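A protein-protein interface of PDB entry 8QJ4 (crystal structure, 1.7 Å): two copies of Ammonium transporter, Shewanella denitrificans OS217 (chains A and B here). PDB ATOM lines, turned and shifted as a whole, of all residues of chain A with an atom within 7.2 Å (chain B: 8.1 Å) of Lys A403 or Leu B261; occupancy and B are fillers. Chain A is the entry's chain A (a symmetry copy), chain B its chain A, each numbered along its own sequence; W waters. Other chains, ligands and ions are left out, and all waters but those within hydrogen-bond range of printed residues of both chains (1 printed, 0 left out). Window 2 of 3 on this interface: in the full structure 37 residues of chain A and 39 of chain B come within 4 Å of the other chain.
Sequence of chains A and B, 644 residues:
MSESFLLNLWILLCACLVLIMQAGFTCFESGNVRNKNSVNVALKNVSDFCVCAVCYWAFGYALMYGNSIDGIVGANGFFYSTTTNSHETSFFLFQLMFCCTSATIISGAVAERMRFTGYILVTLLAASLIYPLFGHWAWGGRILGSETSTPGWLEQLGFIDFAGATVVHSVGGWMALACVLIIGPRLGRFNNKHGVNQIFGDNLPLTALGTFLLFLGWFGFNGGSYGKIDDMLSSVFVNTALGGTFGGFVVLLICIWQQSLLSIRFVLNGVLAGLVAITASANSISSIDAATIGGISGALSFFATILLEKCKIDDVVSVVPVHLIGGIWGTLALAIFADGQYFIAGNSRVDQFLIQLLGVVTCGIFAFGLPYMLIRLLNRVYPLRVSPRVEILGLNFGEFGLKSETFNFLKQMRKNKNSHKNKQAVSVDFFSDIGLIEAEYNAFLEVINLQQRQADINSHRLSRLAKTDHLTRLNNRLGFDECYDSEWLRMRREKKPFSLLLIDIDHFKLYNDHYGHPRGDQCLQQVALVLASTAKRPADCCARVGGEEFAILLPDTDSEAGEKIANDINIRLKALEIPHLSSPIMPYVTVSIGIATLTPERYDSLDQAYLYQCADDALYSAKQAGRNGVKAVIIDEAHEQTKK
The backbone carbonyl oxygen of Phe A400 sits at hydrogen-bond distance from the backbone NH of Leu B262 (3.4 Å).
The backbone carbonyl oxygen (O) of Gly A401 lies within hydrogen-bond range of the backbone NH (N) of Leu B262, at 2.8 Å.
The backbone carbonyl oxygen of Phe A400 lies close to the backbone carbonyl oxygen of Ser B260 (3.5 Å).
N of Ser B263 lies within hydrogen-bond range of O of Phe A400 (2.9 Å).
No position is printed for both chains.
Of the 11 pairs that touch across the chains among the printed residues, none has its exchanged pair printed and touching as well.
O of Asn A396 sits at hydrogen-bond distance from N of Leu A402, at 2.8 Å.
The backbone NH (N) of Ser B260 is in hydrogen-bond range of the backbone carbonyl oxygen (O) of Cys B255, 3.1 Å away.
The backbone carbonyl oxygen (O) of Ser B260 sits at hydrogen-bond distance from the side-chain hydroxyl (OG) of Ser B263 (2.7 Å).
The side-chain hydroxyl (OG) of Ser B263 sits close to the side-chain sulfur (SG) of Cys B255, at 3.6 Å.
O of Cys B255 touches CE1 of Phe A400 (3.6 Å).
Gln B259 touches Phe A400 (CA to CE1, 3.9 Å).
Leu B261 touches Gly A401.
CD2 of Leu A402 touches CE2 of Phe B200 (3.5 Å).
Leu B261 touches Leu A402 (CD1 to CA, 3.96 Å).
CD2 of Leu A402 touches CD1 of Leu B262, 3.9 Å away.
Lys A403 touches Leu B261 (N to CD1, 3.7 Å).
Water W1 lies within hydrogen-bond range of O of Phe A400 (2.7 Å), N of Ile B264 (2.9 Å) and N of Ser B263 (3.2 Å).
Lys A403 touches just one residue of chain B: Leu B261.
Of chain A, only Gly A401 (3.4 Å), Leu A402 (3.96 Å) and Lys A403 (3.7 Å) come within 4 Å of Leu B261.
Of the printed residues of chain A, Gln B259 touches Phe A400 (3.9 Å).
Printed residues of chain A within 4 Å of Leu B262: Phe A400 (3.4 Å), Gly A401 (2.8 Å) and Leu A402 (3.9 Å).
Printed residues of chain A within 4 Å of Cys B255: Phe A400.
Of the printed residues of chain B, Phe A400 touches Cys B255 (3.6 Å), Gln B259 (3.9 Å), Ser B260 (3.5 Å), Leu B262 (3.4 Å) and Ser B263 (2.9 Å).
The nearest residue of chain B that does not touch Lys A403 is Phe B200 (5.9 Å).
The nearest residue of chain A that does not touch Leu B261 is Phe A400 (4.2 Å).
The nearest printed residue of chain A that does not touch Gln B259 is Gly A401 (6.8 Å).
Along chain A the printed residues that touch a printed residue of chain B span positions 400 to 403.
Of the 17 printed residues of chain B, 7 touch a printed residue of chain A.
Hydrophobic or aromatic side chains of chain B within 4 Å of the printed part of chain A: Phe B200, Leu B261 and Leu B262.
Among the printed residues, 11 pairs touch across the chains.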
ATOM      1  N   ASN A 396       6.280 -13.123 -24.577  1.00  0.00           N
ATOM      2  CA  ASN A 396       7.510 -13.874 -24.362  1.00  0.00           C
ATOM      3  C   ASN A 396       8.633 -12.943 -23.852  1.00  0.00           C
ATOM      4  O   ASN A 396       9.552 -13.426 -23.201  1.00  0.00           O
ATOM      5  CB  ASN A 396       8.002 -14.580 -25.625  1.00  0.00           C
ATOM      6  CG  ASN A 396       7.087 -15.675 -26.109  1.00  0.00           C
ATOM      7  OD1 ASN A 396       6.101 -16.009 -25.449  1.00  0.00           O
ATOM      8  ND2 ASN A 396       7.450 -16.282 -27.245  1.00  0.00           N
ATOM      9  N   PHE A 397       8.531 -11.646 -24.179  1.00  0.00           N
ATOM     10  CA  PHE A 397       9.548 -10.660 -23.815  1.00  0.00           C
ATOM     11  C   PHE A 397       9.123  -9.812 -22.618  1.00  0.00           C
ATOM     12  O   PHE A 397       9.689  -8.723 -22.344  1.00  0.00           O
ATOM     13  CB  PHE A 397       9.858  -9.788 -25.033  1.00  0.00           C
ATOM     14  CG  PHE A 397      10.434 -10.556 -26.188  1.00  0.00           C
ATOM     15  CD1 PHE A 397      11.760 -10.952 -26.197  1.00  0.00           C
ATOM     16  CD2 PHE A 397       9.601 -11.020 -27.199  1.00  0.00           C
ATOM     17  CE1 PHE A 397      12.246 -11.726 -27.254  1.00  0.00           C
ATOM     18  CE2 PHE A 397      10.072 -11.835 -28.215  1.00  0.00           C
ATOM     19  CZ  PHE A 397      11.416 -12.151 -28.262  1.00  0.00           C
ATOM     20  N   GLY A 398       8.032 -10.235 -21.972  1.00  0.00           N
ATOM     21  CA  GLY A 398       7.456  -9.509 -20.865  1.00  0.00           C
ATOM     22  C   GLY A 398       8.217  -9.790 -19.573  1.00  0.00           C
ATOM     23  O   GLY A 398       9.352 -10.271 -19.545  1.00  0.00           O
ATOM     24  N   PHE A 400       9.398 -11.624 -16.684  1.00  0.00           N
ATOM     25  CA  PHE A 400       9.790 -12.971 -16.312  1.00  0.00           C
ATOM     26  C   PHE A 400      10.107 -13.812 -17.545  1.00  0.00           C
ATOM     27  O   PHE A 400      10.365 -15.007 -17.416  1.00  0.00           O
ATOM     28  CB  PHE A 400       8.726 -13.620 -15.415  1.00  0.00           C
ATOM     29  CG  PHE A 400       8.350 -12.772 -14.220  1.00  0.00           C
ATOM     30  CD1 PHE A 400       9.310 -12.376 -13.307  1.00  0.00           C
ATOM     31  CD2 PHE A 400       7.082 -12.273 -14.078  1.00  0.00           C
ATOM     32  CE1 PHE A 400       8.993 -11.524 -12.250  1.00  0.00           C
ATOM     33  CE2 PHE A 400       6.772 -11.408 -13.032  1.00  0.00           C
ATOM     34  CZ  PHE A 400       7.722 -11.063 -12.110  1.00  0.00           C
ATOM     35  N   GLY A 401      10.137 -13.179 -18.722  1.00  0.00           N
ATOM     36  CA  GLY A 401      10.380 -13.813 -19.991  1.00  0.00           C
ATOM     37  C   GLY A 401      11.812 -13.614 -20.476  1.00  0.00           C
ATOM     38  O   GLY A 401      12.762 -13.653 -19.693  1.00  0.00           O
ATOM     39  N   LEU A 402      11.957 -13.374 -21.768  1.00  0.00           N
ATOM     40  CA  LEU A 402      13.242 -13.073 -22.386  1.00  0.00           C
ATOM     41  C   LEU A 402      13.578 -11.600 -22.259  1.00  0.00           C
ATOM     42  O   LEU A 402      12.694 -10.768 -22.129  1.00  0.00           O
ATOM     43  CB  LEU A 402      13.193 -13.448 -23.868  1.00  0.00           C
ATOM     44  CG  LEU A 402      13.088 -14.939 -24.143  1.00  0.00           C
ATOM     45  CD1 LEU A 402      12.915 -15.226 -25.642  1.00  0.00           C
ATOM     46  CD2 LEU A 402      14.328 -15.655 -23.610  1.00  0.00           C
ATOM     47  N   LYS A 403      14.875 -11.315 -22.369  1.00  0.00           N
ATOM     48  CA  LYS A 403      15.375  -9.981 -22.653  1.00  0.00           C
ATOM     49  C   LYS A 403      15.109  -9.610 -24.115  1.00  0.00           C
ATOM     50  O   LYS A 403      15.370 -10.384 -25.028  1.00  0.00           O
ATOM     51  CB  LYS A 403      16.874  -9.925 -22.318  1.00  0.00           C
ATOM     52  CG  LYS A 403      17.195  -9.479 -20.898  1.00  0.00           C
ATOM     53  CD  LYS A 403      16.792  -8.035 -20.609  1.00  0.00           C
ATOM     54  CE  LYS A 403      17.395  -7.034 -21.576  1.00  0.00           C
ATOM     55  NZ  LYS A 403      17.055  -5.639 -21.205  1.00  0.00           N
ATOM     56  N   SER A 404      14.544  -8.416 -24.322  1.00  0.00           N
ATOM     57  CA  SER A 404      14.487  -7.834 -25.651  1.00  0.00           C
ATOM     58  C   SER A 404      15.797  -7.084 -25.948  1.00  0.00           C
ATOM     59  O   SER A 404      16.435  -7.442 -26.969  1.00  0.00           O
ATOM     60  CB  SER A 404      13.299  -6.936 -25.785  1.00  0.00           C
ATOM     61  OG  SER A 404      12.948  -6.827 -27.147  1.00  0.00           O
ATOM     62  N   VAL B 196      28.628 -16.371 -18.588  1.00  0.00           N
ATOM     63  CA  VAL B 196      27.612 -17.393 -18.783  1.00  0.00           C
ATOM     64  C   VAL B 196      26.613 -16.859 -19.813  1.00  0.00           C
ATOM     65  O   VAL B 196      26.085 -15.761 -19.654  1.00  0.00           O
ATOM     66  CB  VAL B 196      26.931 -17.773 -17.449  1.00  0.00           C
ATOM     67  CG1 VAL B 196      25.881 -18.849 -17.638  1.00  0.00           C
ATOM     68  CG2 VAL B 196      27.937 -18.242 -16.404  1.00  0.00           C
ATOM     69  N   ASN B 197      26.400 -17.607 -20.909  1.00  0.00           N
ATOM     70  CA  ASN B 197      25.345 -17.286 -21.854  1.00  0.00           C
ATOM     71  C   ASN B 197      24.229 -18.303 -21.663  1.00  0.00           C
ATOM     72  O   ASN B 197      24.509 -19.488 -21.543  1.00  0.00           O
ATOM     73  CB  ASN B 197      25.804 -17.319 -23.308  1.00  0.00           C
ATOM     74  CG  ASN B 197      26.961 -16.376 -23.552  1.00  0.00           C
ATOM     75  OD1 ASN B 197      28.068 -16.793 -23.892  1.00  0.00           O
ATOM     76  ND2 ASN B 197      26.707 -15.098 -23.344  1.00  0.00           N
ATOM     77  N   GLN B 198      22.980 -17.854 -21.668  1.00  0.00           N
ATOM     78  CA  GLN B 198      21.882 -18.785 -21.656  1.00  0.00           C
ATOM     79  C   GLN B 198      21.655 -19.238 -23.094  1.00  0.00           C
ATOM     80  O   GLN B 198      21.800 -18.481 -24.047  1.00  0.00           O
ATOM     81  CB  GLN B 198      20.634 -18.132 -21.056  1.00  0.00           C
ATOM     82  CG  GLN B 198      20.789 -17.769 -19.585  1.00  0.00           C
ATOM     83  CD  GLN B 198      21.133 -18.948 -18.708  1.00  0.00           C
ATOM     84  OE1 GLN B 198      20.636 -20.068 -18.861  1.00  0.00           O
ATOM     85  NE2 GLN B 198      22.051 -18.718 -17.794  1.00  0.00           N
ATOM     86  N   ILE B 199      21.348 -20.519 -23.249  1.00  0.00           N
ATOM     87  CA  ILE B 199      20.930 -21.040 -24.515  1.00  0.00           C
ATOM     88  C   ILE B 199      19.506 -21.558 -24.275  1.00  0.00           C
ATOM     89  O   ILE B 199      19.334 -22.440 -23.452  1.00  0.00           O
ATOM     90  CB  ILE B 199      21.896 -22.147 -24.940  1.00  0.00           C
ATOM     91  CG1 ILE B 199      23.321 -21.610 -25.154  1.00  0.00           C
ATOM     92  CG2 ILE B 199      21.360 -22.849 -26.184  1.00  0.00           C
ATOM     93  CD1 ILE B 199      24.318 -22.712 -25.402  1.00  0.00           C
ATOM     94  N   PHE B 200      18.533 -20.998 -24.960  1.00  0.00           N
ATOM     95  CA  PHE B 200      17.126 -21.246 -24.649  1.00  0.00           C
ATOM     96  C   PHE B 200      16.637 -22.240 -25.704  1.00  0.00           C
ATOM     97  O   PHE B 200      16.940 -22.096 -26.880  1.00  0.00           O
ATOM     98  CB  PHE B 200      16.274 -19.952 -24.724  1.00  0.00           C
ATOM     99  CG  PHE B 200      16.879 -18.687 -24.164  1.00  0.00           C
ATOM    100  CD1 PHE B 200      17.128 -18.572 -22.800  1.00  0.00           C
ATOM    101  CD2 PHE B 200      17.120 -17.589 -24.966  1.00  0.00           C
ATOM    102  CE1 PHE B 200      17.641 -17.395 -22.249  1.00  0.00           C
ATOM    103  CE2 PHE B 200      17.651 -16.420 -24.422  1.00  0.00           C
ATOM    104  CZ  PHE B 200      17.938 -16.328 -23.070  1.00  0.00           C
ATOM    105  N   CYS B 255      11.145 -16.601  -8.395  1.00  0.00           N
ATOM    106  CA  CYS B 255      11.289 -15.932  -9.689  1.00  0.00           C
ATOM    107  C   CYS B 255      10.657 -14.539  -9.630  1.00  0.00           C
ATOM    108  O   CYS B 255      11.185 -13.630 -10.263  1.00  0.00           O
ATOM    109  CB  CYS B 255      10.664 -16.717 -10.841  1.00  0.00           C
ATOM    110  SG  CYS B 255      11.612 -18.220 -11.220  1.00  0.00           S
ATOM    111  N   GLN B 258      13.153 -12.421  -7.579  1.00  0.00           N
ATOM    112  CA  GLN B 258      14.416 -12.200  -8.259  1.00  0.00           C
ATOM    113  C   GLN B 258      14.205 -11.570  -9.635  1.00  0.00           C
ATOM    114  O   GLN B 258      15.174 -11.268 -10.308  1.00  0.00           O
ATOM    115  CB  GLN B 258      15.197 -13.510  -8.376  1.00  0.00           C
ATOM    116  CG  GLN B 258      15.681 -14.088  -7.060  1.00  0.00           C
ATOM    117  CD  GLN B 258      16.845 -13.330  -6.457  1.00  0.00           C
ATOM    118  OE1 GLN B 258      17.871 -13.108  -7.089  1.00  0.00           O
ATOM    119  NE2 GLN B 258      16.699 -12.922  -5.214  1.00  0.00           N
ATOM    120  N   GLN B 259      12.963 -11.415 -10.103  1.00  0.00           N
ATOM    121  CA  GLN B 259      12.735 -11.007 -11.474  1.00  0.00           C
ATOM    122  C   GLN B 259      13.505 -11.875 -12.494  1.00  0.00           C
ATOM    123  O   GLN B 259      14.114 -11.358 -13.406  1.00  0.00           O
ATOM    124  CB  GLN B 259      13.125  -9.529 -11.562  1.00  0.00           C
ATOM    125  CG  GLN B 259      12.443  -8.693 -10.481  1.00  0.00           C
ATOM    126  CD  GLN B 259      12.617  -7.217 -10.739  1.00  0.00           C
ATOM    127  OE1 GLN B 259      11.703  -6.557 -11.212  1.00  0.00           O
ATOM    128  NE2 GLN B 259      13.815  -6.711 -10.504  1.00  0.00           N
ATOM    129  N   SER B 260      13.453 -13.207 -12.369  1.00  0.00           N
ATOM    130  CA  SER B 260      14.316 -14.102 -13.117  1.00  0.00           C
ATOM    131  C   SER B 260      13.936 -14.139 -14.611  1.00  0.00           C
ATOM    132  O   SER B 260      12.767 -14.242 -15.010  1.00  0.00           O
ATOM    133  CB  SER B 260      14.262 -15.486 -12.538  1.00  0.00           C
ATOM    134  OG  SER B 260      14.525 -15.525 -11.135  1.00  0.00           O
ATOM    135  N   LEU B 261      14.979 -14.127 -15.418  1.00  0.00           N
ATOM    136  CA  LEU B 261      14.958 -14.323 -16.857  1.00  0.00           C
ATOM    137  C   LEU B 261      14.459 -15.739 -17.137  1.00  0.00           C
ATOM    138  O   LEU B 261      14.859 -16.704 -16.475  1.00  0.00           O
ATOM    139  CB  LEU B 261      16.399 -14.150 -17.374  1.00  0.00           C
ATOM    140  CG  LEU B 261      16.677 -14.612 -18.805  1.00  0.00           C
ATOM    141  CD1 LEU B 261      16.201 -13.554 -19.805  1.00  0.00           C
ATOM    142  CD2 LEU B 261      18.174 -14.927 -19.006  1.00  0.00           C
ATOM    143  N   LEU B 262      13.544 -15.843 -18.095  1.00  0.00           N
ATOM    144  CA  LEU B 262      13.023 -17.153 -18.484  1.00  0.00           C
ATOM    145  C   LEU B 262      12.645 -17.989 -17.256  1.00  0.00           C
ATOM    146  O   LEU B 262      13.009 -19.151 -17.077  1.00  0.00           O
ATOM    147  CB  LEU B 262      14.016 -17.773 -19.472  1.00  0.00           C
ATOM    148  CG  LEU B 262      13.373 -18.588 -20.607  1.00  0.00           C
ATOM    149  CD1 LEU B 262      12.190 -17.885 -21.304  1.00  0.00           C
ATOM    150  CD2 LEU B 262      14.424 -18.966 -21.620  1.00  0.00           C
ATOM    151  N   SER B 263      11.800 -17.368 -16.411  1.00  0.00           N
ATOM    152  CA  SER B 263      11.239 -17.999 -15.246  1.00  0.00           C
ATOM    153  C   SER B 263      10.564 -19.340 -15.581  1.00  0.00           C
ATOM    154  O   SER B 263      10.541 -20.206 -14.755  1.00  0.00           O
ATOM    155  CB  SER B 263      10.251 -17.070 -14.556  1.00  0.00           C
ATOM    156  OG  SER B 263      10.952 -15.959 -13.940  1.00  0.00           O
ATOM    157  N   ILE B 264       9.939 -19.456 -16.766  1.00  0.00           N
ATOM    158  CA  ILE B 264       9.229 -20.699 -17.073  1.00  0.00           C
ATOM    159  C   ILE B 264      10.115 -21.927 -16.835  1.00  0.00           C
ATOM    160  O   ILE B 264       9.665 -22.943 -16.262  1.00  0.00           O
ATOM    161  CB  ILE B 264       8.612 -20.686 -18.469  1.00  0.00           C
ATOM    162  CG1 ILE B 264       7.645 -21.889 -18.597  1.00  0.00           C
ATOM    163  CG2 ILE B 264       9.693 -20.623 -19.517  1.00  0.00           C
ATOM    164  CD1 ILE B 264       7.010 -21.961 -19.919  1.00  0.00           C
ATOM    165  N   ARG B 265      11.375 -21.854 -17.240  1.00  0.00           N
ATOM    166  CA  ARG B 265      12.226 -23.027 -17.106  1.00  0.00           C
ATOM    167  C   ARG B 265      12.474 -23.386 -15.626  1.00  0.00           C
ATOM    168  O   ARG B 265      12.397 -24.568 -15.204  1.00  0.00           O
ATOM    169  CB  ARG B 265      13.563 -22.808 -17.808  1.00  0.00           C
ATOM    170  CG  ARG B 265      13.442 -22.504 -19.295  1.00  0.00           C
ATOM    171  CD  ARG B 265      14.754 -22.779 -20.002  1.00  0.00           C
ATOM    172  NE  ARG B 265      15.852 -21.981 -19.440  1.00  0.00           N
ATOM    173  CZ  ARG B 265      17.087 -21.910 -19.976  1.00  0.00           C
ATOM    174  NH1 ARG B 265      17.387 -22.647 -21.043  1.00  0.00           N
ATOM    175  NH2 ARG B 265      17.989 -21.050 -19.467  1.00  0.00           N
ATOM    176  N   PHE B 266      12.661 -22.356 -14.806  1.00  0.00           N
ATOM    177  CA  PHE B 266      12.866 -22.621 -13.384  1.00  0.00           C
ATOM    178  C   PHE B 266      11.602 -23.166 -12.747  1.00  0.00           C
ATOM    179  O   PHE B 266      11.666 -24.103 -11.943  1.00  0.00           O
ATOM    180  CB  PHE B 266      13.193 -21.302 -12.654  1.00  0.00           C
ATOM    181  CG  PHE B 266      14.580 -20.771 -12.866  1.00  0.00           C
ATOM    182  CD1 PHE B 266      15.674 -21.395 -12.275  1.00  0.00           C
ATOM    183  CD2 PHE B 266      14.802 -19.607 -13.576  1.00  0.00           C
ATOM    184  CE1 PHE B 266      16.966 -20.894 -12.468  1.00  0.00           C
ATOM    185  CE2 PHE B 266      16.095 -19.110 -13.778  1.00  0.00           C
ATOM    186  CZ  PHE B 266      17.179 -19.769 -13.238  1.00  0.00           C
ATOM    187  N   PHE B 302      16.350 -24.452  -7.903  1.00  0.00           N
ATOM    188  CA  PHE B 302      16.637 -23.107  -8.385  1.00  0.00           C
ATOM    189  C   PHE B 302      18.105 -22.753  -8.087  1.00  0.00           C
ATOM    190  O   PHE B 302      18.885 -22.385  -8.962  1.00  0.00           O
ATOM    191  CB  PHE B 302      15.674 -22.092  -7.750  1.00  0.00           C
ATOM    192  CG  PHE B 302      15.892 -20.655  -8.168  1.00  0.00           C
ATOM    193  CD1 PHE B 302      16.813 -19.854  -7.496  1.00  0.00           C
ATOM    194  CD2 PHE B 302      15.208 -20.098  -9.243  1.00  0.00           C
ATOM    195  CE1 PHE B 302      17.070 -18.549  -7.915  1.00  0.00           C
ATOM    196  CE2 PHE B 302      15.444 -18.785  -9.653  1.00  0.00           C
ATOM    197  CZ  PHE B 302      16.383 -18.004  -8.985  1.00  0.00           C
ATOM    198  N   GLU B 309      26.108 -23.527 -13.099  1.00  0.00           N
ATOM    199  CA  GLU B 309      26.620 -22.546 -14.031  1.00  0.00           C
ATOM    200  C   GLU B 309      27.917 -21.930 -13.513  1.00  0.00           C
ATOM    201  O   GLU B 309      28.856 -21.779 -14.284  1.00  0.00           O
ATOM    202  CB  GLU B 309      25.653 -21.385 -14.232  1.00  0.00           C
ATOM    203  CG  GLU B 309      24.504 -21.689 -15.125  1.00  0.00           C
ATOM    204  CD  GLU B 309      23.679 -20.441 -15.390  1.00  0.00           C
ATOM    205  OE1 GLU B 309      23.025 -20.427 -16.444  1.00  0.00           O
ATOM    206  OE2 GLU B 309      23.705 -19.488 -14.553  1.00  0.00           O
HETATM  207  O   HOH W   1       9.432 -17.287 -18.593  1.00  0.00           O
